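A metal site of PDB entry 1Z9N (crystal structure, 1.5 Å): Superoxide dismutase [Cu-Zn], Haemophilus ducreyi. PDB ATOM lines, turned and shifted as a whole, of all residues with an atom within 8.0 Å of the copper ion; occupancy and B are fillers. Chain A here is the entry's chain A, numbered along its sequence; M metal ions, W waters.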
ATOM      1  N   GLY A  68       4.319  -8.671   0.547  1.00  0.00           N
ATOM      2  CA  GLY A  68       4.377  -9.482   1.766  1.00  0.00           C
ATOM      3  C   GLY A  68       3.777  -8.719   2.943  1.00  0.00           C
ATOM      4  O   GLY A  68       4.010  -7.519   3.111  1.00  0.00           O
ATOM      5  N   PHE A  69       3.066  -9.440   3.783  1.00  0.00           N
ATOM      6  CA  PHE A  69       2.207  -8.926   4.840  1.00  0.00           C
ATOM      7  C   PHE A  69       2.289  -9.910   5.974  1.00  0.00           C
ATOM      8  O   PHE A  69       1.812 -11.068   5.835  1.00  0.00           O
ATOM      9  CB  PHE A  69       0.802  -8.826   4.251  1.00  0.00           C
ATOM     10  CG  PHE A  69      -0.218  -8.112   5.102  1.00  0.00           C
ATOM     11  CD1 PHE A  69       0.090  -6.964   5.810  1.00  0.00           C
ATOM     12  CD2 PHE A  69      -1.530  -8.555   5.113  1.00  0.00           C
ATOM     13  CE1 PHE A  69      -0.874  -6.298   6.530  1.00  0.00           C
ATOM     14  CE2 PHE A  69      -2.498  -7.906   5.836  1.00  0.00           C
ATOM     15  CZ  PHE A  69      -2.195  -6.770   6.538  1.00  0.00           C
ATOM     16  N   HIS A  70       3.000  -9.524   7.041  1.00  0.00           N
ATOM     17  CA  HIS A  70       3.209 -10.412   8.169  1.00  0.00           C
ATOM     18  C   HIS A  70       3.133  -9.678   9.490  1.00  0.00           C
ATOM     19  O   HIS A  70       3.375  -8.465   9.550  1.00  0.00           O
ATOM     20  CB  HIS A  70       4.595 -11.119   8.125  1.00  0.00           C
ATOM     21  CG  HIS A  70       5.169 -11.285   6.763  1.00  0.00           C
ATOM     22  ND1 HIS A  70       6.199 -10.483   6.271  1.00  0.00           N
ATOM     23  CD2 HIS A  70       4.813 -12.105   5.746  1.00  0.00           C
ATOM     24  CE1 HIS A  70       6.476 -10.851   5.032  1.00  0.00           C
ATOM     25  NE2 HIS A  70       5.643 -11.824   4.684  1.00  0.00           N
ATOM     26  N   ILE A  71       2.800 -10.440  10.539  1.00  0.00           N
ATOM     27  CA  ILE A  71       2.945  -9.968  11.894  1.00  0.00           C
ATOM     28  C   ILE A  71       4.387 -10.250  12.313  1.00  0.00           C
ATOM     29  O   ILE A  71       4.912 -11.373  12.150  1.00  0.00           O
ATOM     30  CB  ILE A  71       1.959 -10.638  12.825  1.00  0.00           C
ATOM     31  CG1 ILE A  71       0.529 -10.340  12.369  1.00  0.00           C
ATOM     32  CG2 ILE A  71       2.165 -10.121  14.261  1.00  0.00           C
ATOM     33  CD1 ILE A  71      -0.473 -11.177  13.093  1.00  0.00           C
ATOM     34  N   HIS A  72       5.043  -9.213  12.839  1.00  0.00           N
ATOM     35  CA  HIS A  72       6.405  -9.354  13.360  1.00  0.00           C
ATOM     36  C   HIS A  72       6.397  -9.357  14.879  1.00  0.00           C
ATOM     37  O   HIS A  72       5.421  -8.976  15.511  1.00  0.00           O
ATOM     38  CB  HIS A  72       7.303  -8.249  12.809  1.00  0.00           C
ATOM     39  CG  HIS A  72       7.703  -8.449  11.387  1.00  0.00           C
ATOM     40  ND1 HIS A  72       9.015  -8.470  10.948  1.00  0.00           N
ATOM     41  CD2 HIS A  72       6.940  -8.662  10.280  1.00  0.00           C
ATOM     42  CE1 HIS A  72       9.034  -8.664   9.628  1.00  0.00           C
ATOM     43  NE2 HIS A  72       7.790  -8.798   9.215  1.00  0.00           N
ATOM     44  N   ALA A  92      11.138  -3.856  14.541  1.00  0.00           N
ATOM     45  CA  ALA A  92      10.042  -4.820  14.694  1.00  0.00           C
ATOM     46  C   ALA A  92      10.512  -6.265  14.878  1.00  0.00           C
ATOM     47  O   ALA A  92       9.748  -7.152  15.284  1.00  0.00           O
ATOM     48  CB  ALA A  92       9.165  -4.735  13.468  1.00  0.00           C
ATOM     49  N   GLY A  93      11.774  -6.518  14.586  1.00  0.00           N
ATOM     50  CA  GLY A  93      12.316  -7.864  14.698  1.00  0.00           C
ATOM     51  C   GLY A  93      11.816  -8.764  13.594  1.00  0.00           C
ATOM     52  O   GLY A  93      11.417  -8.290  12.527  1.00  0.00           O
ATOM     53  N   GLY A  94      11.828 -10.058  13.861  1.00  0.00           N
ATOM     54  CA  GLY A  94      11.547 -11.061  12.855  1.00  0.00           C
ATOM     55  C   GLY A  94      10.072 -11.349  12.762  1.00  0.00           C
ATOM     56  O   GLY A  94       9.240 -10.749  13.443  1.00  0.00           O
ATOM     57  N   HIS A  95       9.743 -12.275  11.891  1.00  0.00           N
ATOM     58  CA  HIS A  95       8.349 -12.713  11.804  1.00  0.00           C
ATOM     59  C   HIS A  95       7.924 -13.289  13.140  1.00  0.00           C
ATOM     60  O   HIS A  95       8.694 -13.993  13.843  1.00  0.00           O
ATOM     61  CB  HIS A  95       8.208 -13.763  10.689  1.00  0.00           C
ATOM     62  CG  HIS A  95       8.393 -13.227   9.301  1.00  0.00           C
ATOM     63  ND1 HIS A  95       7.864 -13.819   8.173  1.00  0.00           N
ATOM     64  CD2 HIS A  95       9.004 -12.086   8.879  1.00  0.00           C
ATOM     65  CE1 HIS A  95       8.199 -13.101   7.112  1.00  0.00           C
ATOM     66  NE2 HIS A  95       8.908 -12.063   7.511  1.00  0.00           N
ATOM     67  N   TRP A  96       6.692 -12.988  13.539  1.00  0.00           N
ATOM     68  CA  TRP A  96       6.135 -13.524  14.774  1.00  0.00           C
ATOM     69  C   TRP A  96       6.057 -15.036  14.682  1.00  0.00           C
ATOM     70  O   TRP A  96       5.365 -15.595  13.828  1.00  0.00           O
ATOM     71  CB  TRP A  96       4.796 -12.872  15.060  1.00  0.00           C
ATOM     72  CG  TRP A  96       4.121 -13.351  16.296  1.00  0.00           C
ATOM     73  CD1 TRP A  96       4.678 -13.510  17.533  1.00  0.00           C
ATOM     74  CD2 TRP A  96       2.755 -13.690  16.412  1.00  0.00           C
ATOM     75  NE1 TRP A  96       3.715 -13.960  18.402  1.00  0.00           N
ATOM     76  CE2 TRP A  96       2.524 -14.074  17.736  1.00  0.00           C
ATOM     77  CE3 TRP A  96       1.685 -13.692  15.496  1.00  0.00           C
ATOM     78  CZ2 TRP A  96       1.274 -14.495  18.192  1.00  0.00           C
ATOM     79  CZ3 TRP A  96       0.457 -14.128  15.933  1.00  0.00           C
ATOM     80  CH2 TRP A  96       0.252 -14.489  17.292  1.00  0.00           C
ATOM     81  N   HIS A 104       9.284 -19.815   7.170  1.00  0.00           N
ATOM     82  CA  HIS A 104       8.246 -18.972   6.549  1.00  0.00           C
ATOM     83  C   HIS A 104       7.360 -19.844   5.663  1.00  0.00           C
ATOM     84  O   HIS A 104       7.853 -20.716   4.953  1.00  0.00           O
ATOM     85  CB  HIS A 104       8.875 -17.858   5.735  1.00  0.00           C
ATOM     86  CG  HIS A 104       7.895 -16.903   5.164  1.00  0.00           C
ATOM     87  ND1 HIS A 104       7.188 -16.034   5.968  1.00  0.00           N
ATOM     88  CD2 HIS A 104       7.480 -16.720   3.902  1.00  0.00           C
ATOM     89  CE1 HIS A 104       6.344 -15.371   5.187  1.00  0.00           C
ATOM     90  NE2 HIS A 104       6.509 -15.758   3.929  1.00  0.00           N
ATOM     91  N   HIS A 113       5.418 -19.619  10.264  1.00  0.00           N
ATOM     92  CA  HIS A 113       5.338 -18.651  11.327  1.00  0.00           C
ATOM     93  C   HIS A 113       3.873 -18.248  11.592  1.00  0.00           C
ATOM     94  O   HIS A 113       3.122 -18.032  10.664  1.00  0.00           O
ATOM     95  CB  HIS A 113       6.032 -17.345  10.937  1.00  0.00           C
ATOM     96  CG  HIS A 113       7.460 -17.484  10.533  1.00  0.00           C
ATOM     97  ND1 HIS A 113       7.981 -16.845   9.423  1.00  0.00           N
ATOM     98  CD2 HIS A 113       8.513 -18.106  11.126  1.00  0.00           C
ATOM     99  CE1 HIS A 113       9.275 -17.101   9.334  1.00  0.00           C
ATOM    100  NE2 HIS A 113       9.617 -17.860  10.358  1.00  0.00           N
ATOM    101  N   GLY A 115       2.783 -15.504  12.310  1.00  0.00           N
ATOM    102  CA  GLY A 115       2.560 -14.219  11.711  1.00  0.00           C
ATOM    103  C   GLY A 115       2.382 -14.142  10.203  1.00  0.00           C
ATOM    104  O   GLY A 115       2.221 -13.070   9.680  1.00  0.00           O
ATOM    105  N   ASP A 116       2.459 -15.269   9.510  1.00  0.00           N
ATOM    106  CA  ASP A 116       2.387 -15.299   8.054  1.00  0.00           C
ATOM    107  C   ASP A 116       0.966 -15.131   7.537  1.00  0.00           C
ATOM    108  O   ASP A 116       0.141 -16.044   7.736  1.00  0.00           O
ATOM    109  CB  ASP A 116       2.999 -16.605   7.571  1.00  0.00           C
ATOM    110  CG  ASP A 116       4.478 -16.656   7.808  1.00  0.00           C
ATOM    111  OD1 ASP A 116       5.038 -15.576   8.130  1.00  0.00           O
ATOM    112  OD2 ASP A 116       5.138 -17.699   7.628  1.00  0.00           O
ATOM    113  N   SER A 147       3.720  -6.280  15.758  1.00  0.00           N
ATOM    114  CA  SER A 147       3.682  -5.290  14.706  1.00  0.00           C
ATOM    115  C   SER A 147       3.157  -5.894  13.400  1.00  0.00           C
ATOM    116  O   SER A 147       3.260  -7.106  13.185  1.00  0.00           O
ATOM    117  CB  SER A 147       5.060  -4.677  14.467  1.00  0.00           C
ATOM    118  OG  SER A 147       6.037  -5.686  14.323  1.00  0.00           O
ATOM    119  N   LEU A 148       2.517  -5.050  12.589  1.00  0.00           N
ATOM    120  CA  LEU A 148       1.985  -5.455  11.291  1.00  0.00           C
ATOM    121  C   LEU A 148       2.828  -4.814  10.210  1.00  0.00           C
ATOM    122  O   LEU A 148       2.962  -3.594  10.139  1.00  0.00           O
ATOM    123  CB  LEU A 148       0.553  -4.973  11.176  1.00  0.00           C
ATOM    124  CG  LEU A 148      -0.231  -5.479   9.988  1.00  0.00           C
ATOM    125  CD1 LEU A 148      -0.349  -6.985  10.003  1.00  0.00           C
ATOM    126  CD2 LEU A 148      -1.607  -4.806   9.966  1.00  0.00           C
ATOM    127  N   MET A 149       3.413  -5.643   9.362  1.00  0.00           N
ATOM    128  CA  MET A 149       4.415  -5.165   8.416  1.00  0.00           C
ATOM    129  C   MET A 149       3.958  -5.415   6.973  1.00  0.00           C
ATOM    130  O   MET A 149       3.438  -6.490   6.664  1.00  0.00           O
ATOM    131  CB  MET A 149       5.732  -5.924   8.665  1.00  0.00           C
ATOM    132  CG  MET A 149       6.996  -5.368   8.031  1.00  0.00           C
ATOM    133  SD  MET A 149       7.472  -3.841   8.832  1.00  0.00           S
ATOM    134  CE  MET A 149       8.046  -4.442  10.408  1.00  0.00           C
ATOM    135  N   ILE A 150       4.176  -4.435   6.105  1.00  0.00           N
ATOM    136  CA  ILE A 150       3.987  -4.566   4.676  1.00  0.00           C
ATOM    137  C   ILE A 150       5.338  -4.325   4.026  1.00  0.00           C
ATOM    138  O   ILE A 150       6.008  -3.312   4.264  1.00  0.00           O
ATOM    139  CB  ILE A 150       2.969  -3.544   4.177  1.00  0.00           C
ATOM    140  CG1 ILE A 150       1.695  -3.578   5.031  1.00  0.00           C
ATOM    141  CG2 ILE A 150       2.655  -3.796   2.708  1.00  0.00           C
ATOM    142  CD1 ILE A 150       0.718  -2.447   4.706  1.00  0.00           C
ATOM    143  N   HIS A 151       5.739  -5.267   3.176  1.00  0.00           N
ATOM    144  CA  HIS A 151       7.048  -5.215   2.560  1.00  0.00           C
ATOM    145  C   HIS A 151       6.989  -4.624   1.174  1.00  0.00           C
ATOM    146  O   HIS A 151       5.949  -4.586   0.520  1.00  0.00           O
ATOM    147  CB  HIS A 151       7.575  -6.630   2.498  1.00  0.00           C
ATOM    148  CG  HIS A 151       7.914  -7.171   3.849  1.00  0.00           C
ATOM    149  ND1 HIS A 151       9.193  -7.139   4.365  1.00  0.00           N
ATOM    150  CD2 HIS A 151       7.130  -7.733   4.812  1.00  0.00           C
ATOM    151  CE1 HIS A 151       9.192  -7.681   5.574  1.00  0.00           C
ATOM    152  NE2 HIS A 151       7.943  -8.033   5.886  1.00  0.00           N
ATOM    153  N   ASP A 155       5.360 -12.169  -1.685  1.00  0.00           N
ATOM    154  CA  ASP A 155       5.433 -13.281  -0.770  1.00  0.00           C
ATOM    155  C   ASP A 155       5.055 -14.558  -1.491  1.00  0.00           C
ATOM    156  O   ASP A 155       3.895 -14.785  -1.786  1.00  0.00           O
ATOM    157  CB  ASP A 155       4.500 -13.066   0.432  1.00  0.00           C
ATOM    158  CG  ASP A 155       4.855 -13.923   1.642  1.00  0.00           C
ATOM    159  OD1 ASP A 155       5.578 -14.950   1.504  1.00  0.00           O
ATOM    160  OD2 ASP A 155       4.389 -13.646   2.765  1.00  0.00           O
ATOM    161  N   LEU A 164      12.077 -15.536   3.693  1.00  0.00           N
ATOM    162  CA  LEU A 164      10.914 -14.818   4.195  1.00  0.00           C
ATOM    163  C   LEU A 164       9.989 -14.399   3.064  1.00  0.00           C
ATOM    164  O   LEU A 164       9.367 -13.324   3.112  1.00  0.00           O
ATOM    165  CB  LEU A 164      11.341 -13.651   5.072  1.00  0.00           C
ATOM    166  CG  LEU A 164      12.134 -14.134   6.308  1.00  0.00           C
ATOM    167  CD1 LEU A 164      12.640 -12.914   7.040  1.00  0.00           C
ATOM    168  CD2 LEU A 164      11.359 -15.049   7.236  1.00  0.00           C
ATOM    169  N   GLY A 167       9.959 -10.865   0.642  1.00  0.00           N
ATOM    170  CA  GLY A 167       9.432  -9.568   1.073  1.00  0.00           C
ATOM    171  C   GLY A 167      10.450  -8.423   0.930  1.00  0.00           C
ATOM    172  O   GLY A 167      10.136  -7.325   0.516  1.00  0.00           O
ATOM    173  N   GLY A 168      11.669  -8.684   1.389  1.00  0.00           N
ATOM    174  CA  GLY A 168      12.701  -7.681   1.281  1.00  0.00           C
ATOM    175  C   GLY A 168      12.409  -6.543   2.226  1.00  0.00           C
ATOM    176  O   GLY A 168      11.949  -6.780   3.362  1.00  0.00           O
ATOM    177  N   PRO A 169      12.695  -5.330   1.782  1.00  0.00           N
ATOM    178  CA  PRO A 169      12.590  -4.156   2.639  1.00  0.00           C
ATOM    179  C   PRO A 169      11.210  -3.984   3.244  1.00  0.00           C
ATOM    180  O   PRO A 169      10.214  -4.406   2.666  1.00  0.00           O
ATOM    181  CB  PRO A 169      12.838  -3.023   1.672  1.00  0.00           C
ATOM    182  CG  PRO A 169      13.738  -3.561   0.681  1.00  0.00           C
ATOM    183  CD  PRO A 169      13.245  -4.971   0.460  1.00  0.00           C
ATOM    184  N   ARG A 170      11.182  -3.323   4.376  1.00  0.00           N
ATOM    185  CA  ARG A 170       9.954  -3.033   5.100  1.00  0.00           C
ATOM    186  C   ARG A 170       9.438  -1.670   4.665  1.00  0.00           C
ATOM    187  O   ARG A 170      10.062  -0.629   4.941  1.00  0.00           O
ATOM    188  CB  ARG A 170      10.268  -3.124   6.597  1.00  0.00           C
ATOM    189  CG  ARG A 170      10.807  -4.496   7.004  1.00  0.00           C
ATOM    190  CD  ARG A 170      11.456  -4.595   8.353  1.00  0.00           C
ATOM    191  NE  ARG A 170      11.989  -5.941   8.546  1.00  0.00           N
ATOM    192  CZ  ARG A 170      12.090  -6.578   9.711  1.00  0.00           C
ATOM    193  NH1 ARG A 170      11.740  -6.037  10.864  1.00  0.00           N
ATOM    194  NH2 ARG A 170      12.570  -7.811   9.716  1.00  0.00           N
ATOM    195  N   ALA A 172       5.990  -0.409   5.024  1.00  0.00           N
ATOM    196  CA  ALA A 172       5.019   0.214   5.904  1.00  0.00           C
ATOM    197  C   ALA A 172       4.763  -0.679   7.129  1.00  0.00           C
ATOM    198  O   ALA A 172       4.964  -1.893   7.071  1.00  0.00           O
ATOM    199  CB  ALA A 172       3.742   0.480   5.163  1.00  0.00           C
HETATM  200 CU    CU M   1       7.340  -9.245   7.343  1.00  0.00          CU
HETATM  201 ZN    ZN M   2       7.033 -15.689   8.003  1.00  0.00          ZN
HETATM  202  O   HOH W   1      10.494 -10.082   6.881  1.00  0.00           O
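The backbone carbonyl oxygen of Gly 94 lies close to a ring nitrogen (ND1) of His 72 (3.4 Å).
A ring nitrogen (ND1) of His 72 lies within hydrogen-bond range of the backbone carbonyl oxygen (O) of Gly 93, at 2.9 Å.
The backbone NH (N) of His 72 lies within hydrogen-bond range of the backbone carbonyl oxygen (O) of Ser 147, at 2.8 Å.
The backbone carbonyl oxygen of Gly 68 sits at hydrogen-bond distance from the backbone NH of His 151, at 2.8 Å.
The backbone carbonyl oxygen of Gly 168 sits at hydrogen-bond distance from a ring nitrogen (ND1) of His 151.
ND1 of His 70 sits close to NE2 of His 95 (3.4 Å).
The backbone NH of Met 149 lies within hydrogen-bond range of the backbone carbonyl oxygen of His 70 (2.8 Å).
The side-chain carboxylate of Asp 155 sits at hydrogen-bond distance from a ring nitrogen (NE2) of His 70 (2.9 Å).
NE2 of His 95 touches the copper ion, at 3.2 Å.
Met 149 touches the copper ion (CB to CU, 3.9 Å).
Within 4 Å of the copper ion: His 70, His 72, His 95, Met 149 and His 151.
Along chain A the residues within 4 Å of the copper ion span positions 70 to 151.
The nearest printed residue that does not touch the copper ion is Phe 69 (5.3 Å).
The copper ion is bound by a ring nitrogen (NE2) of His 72 (2.0 Å), a ring nitrogen (NE2) of His 151 (2.0 Å) and a ring nitrogen (ND1) of His 70 (2.0 Å).
The copper ion has three donor atoms within binding distance.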
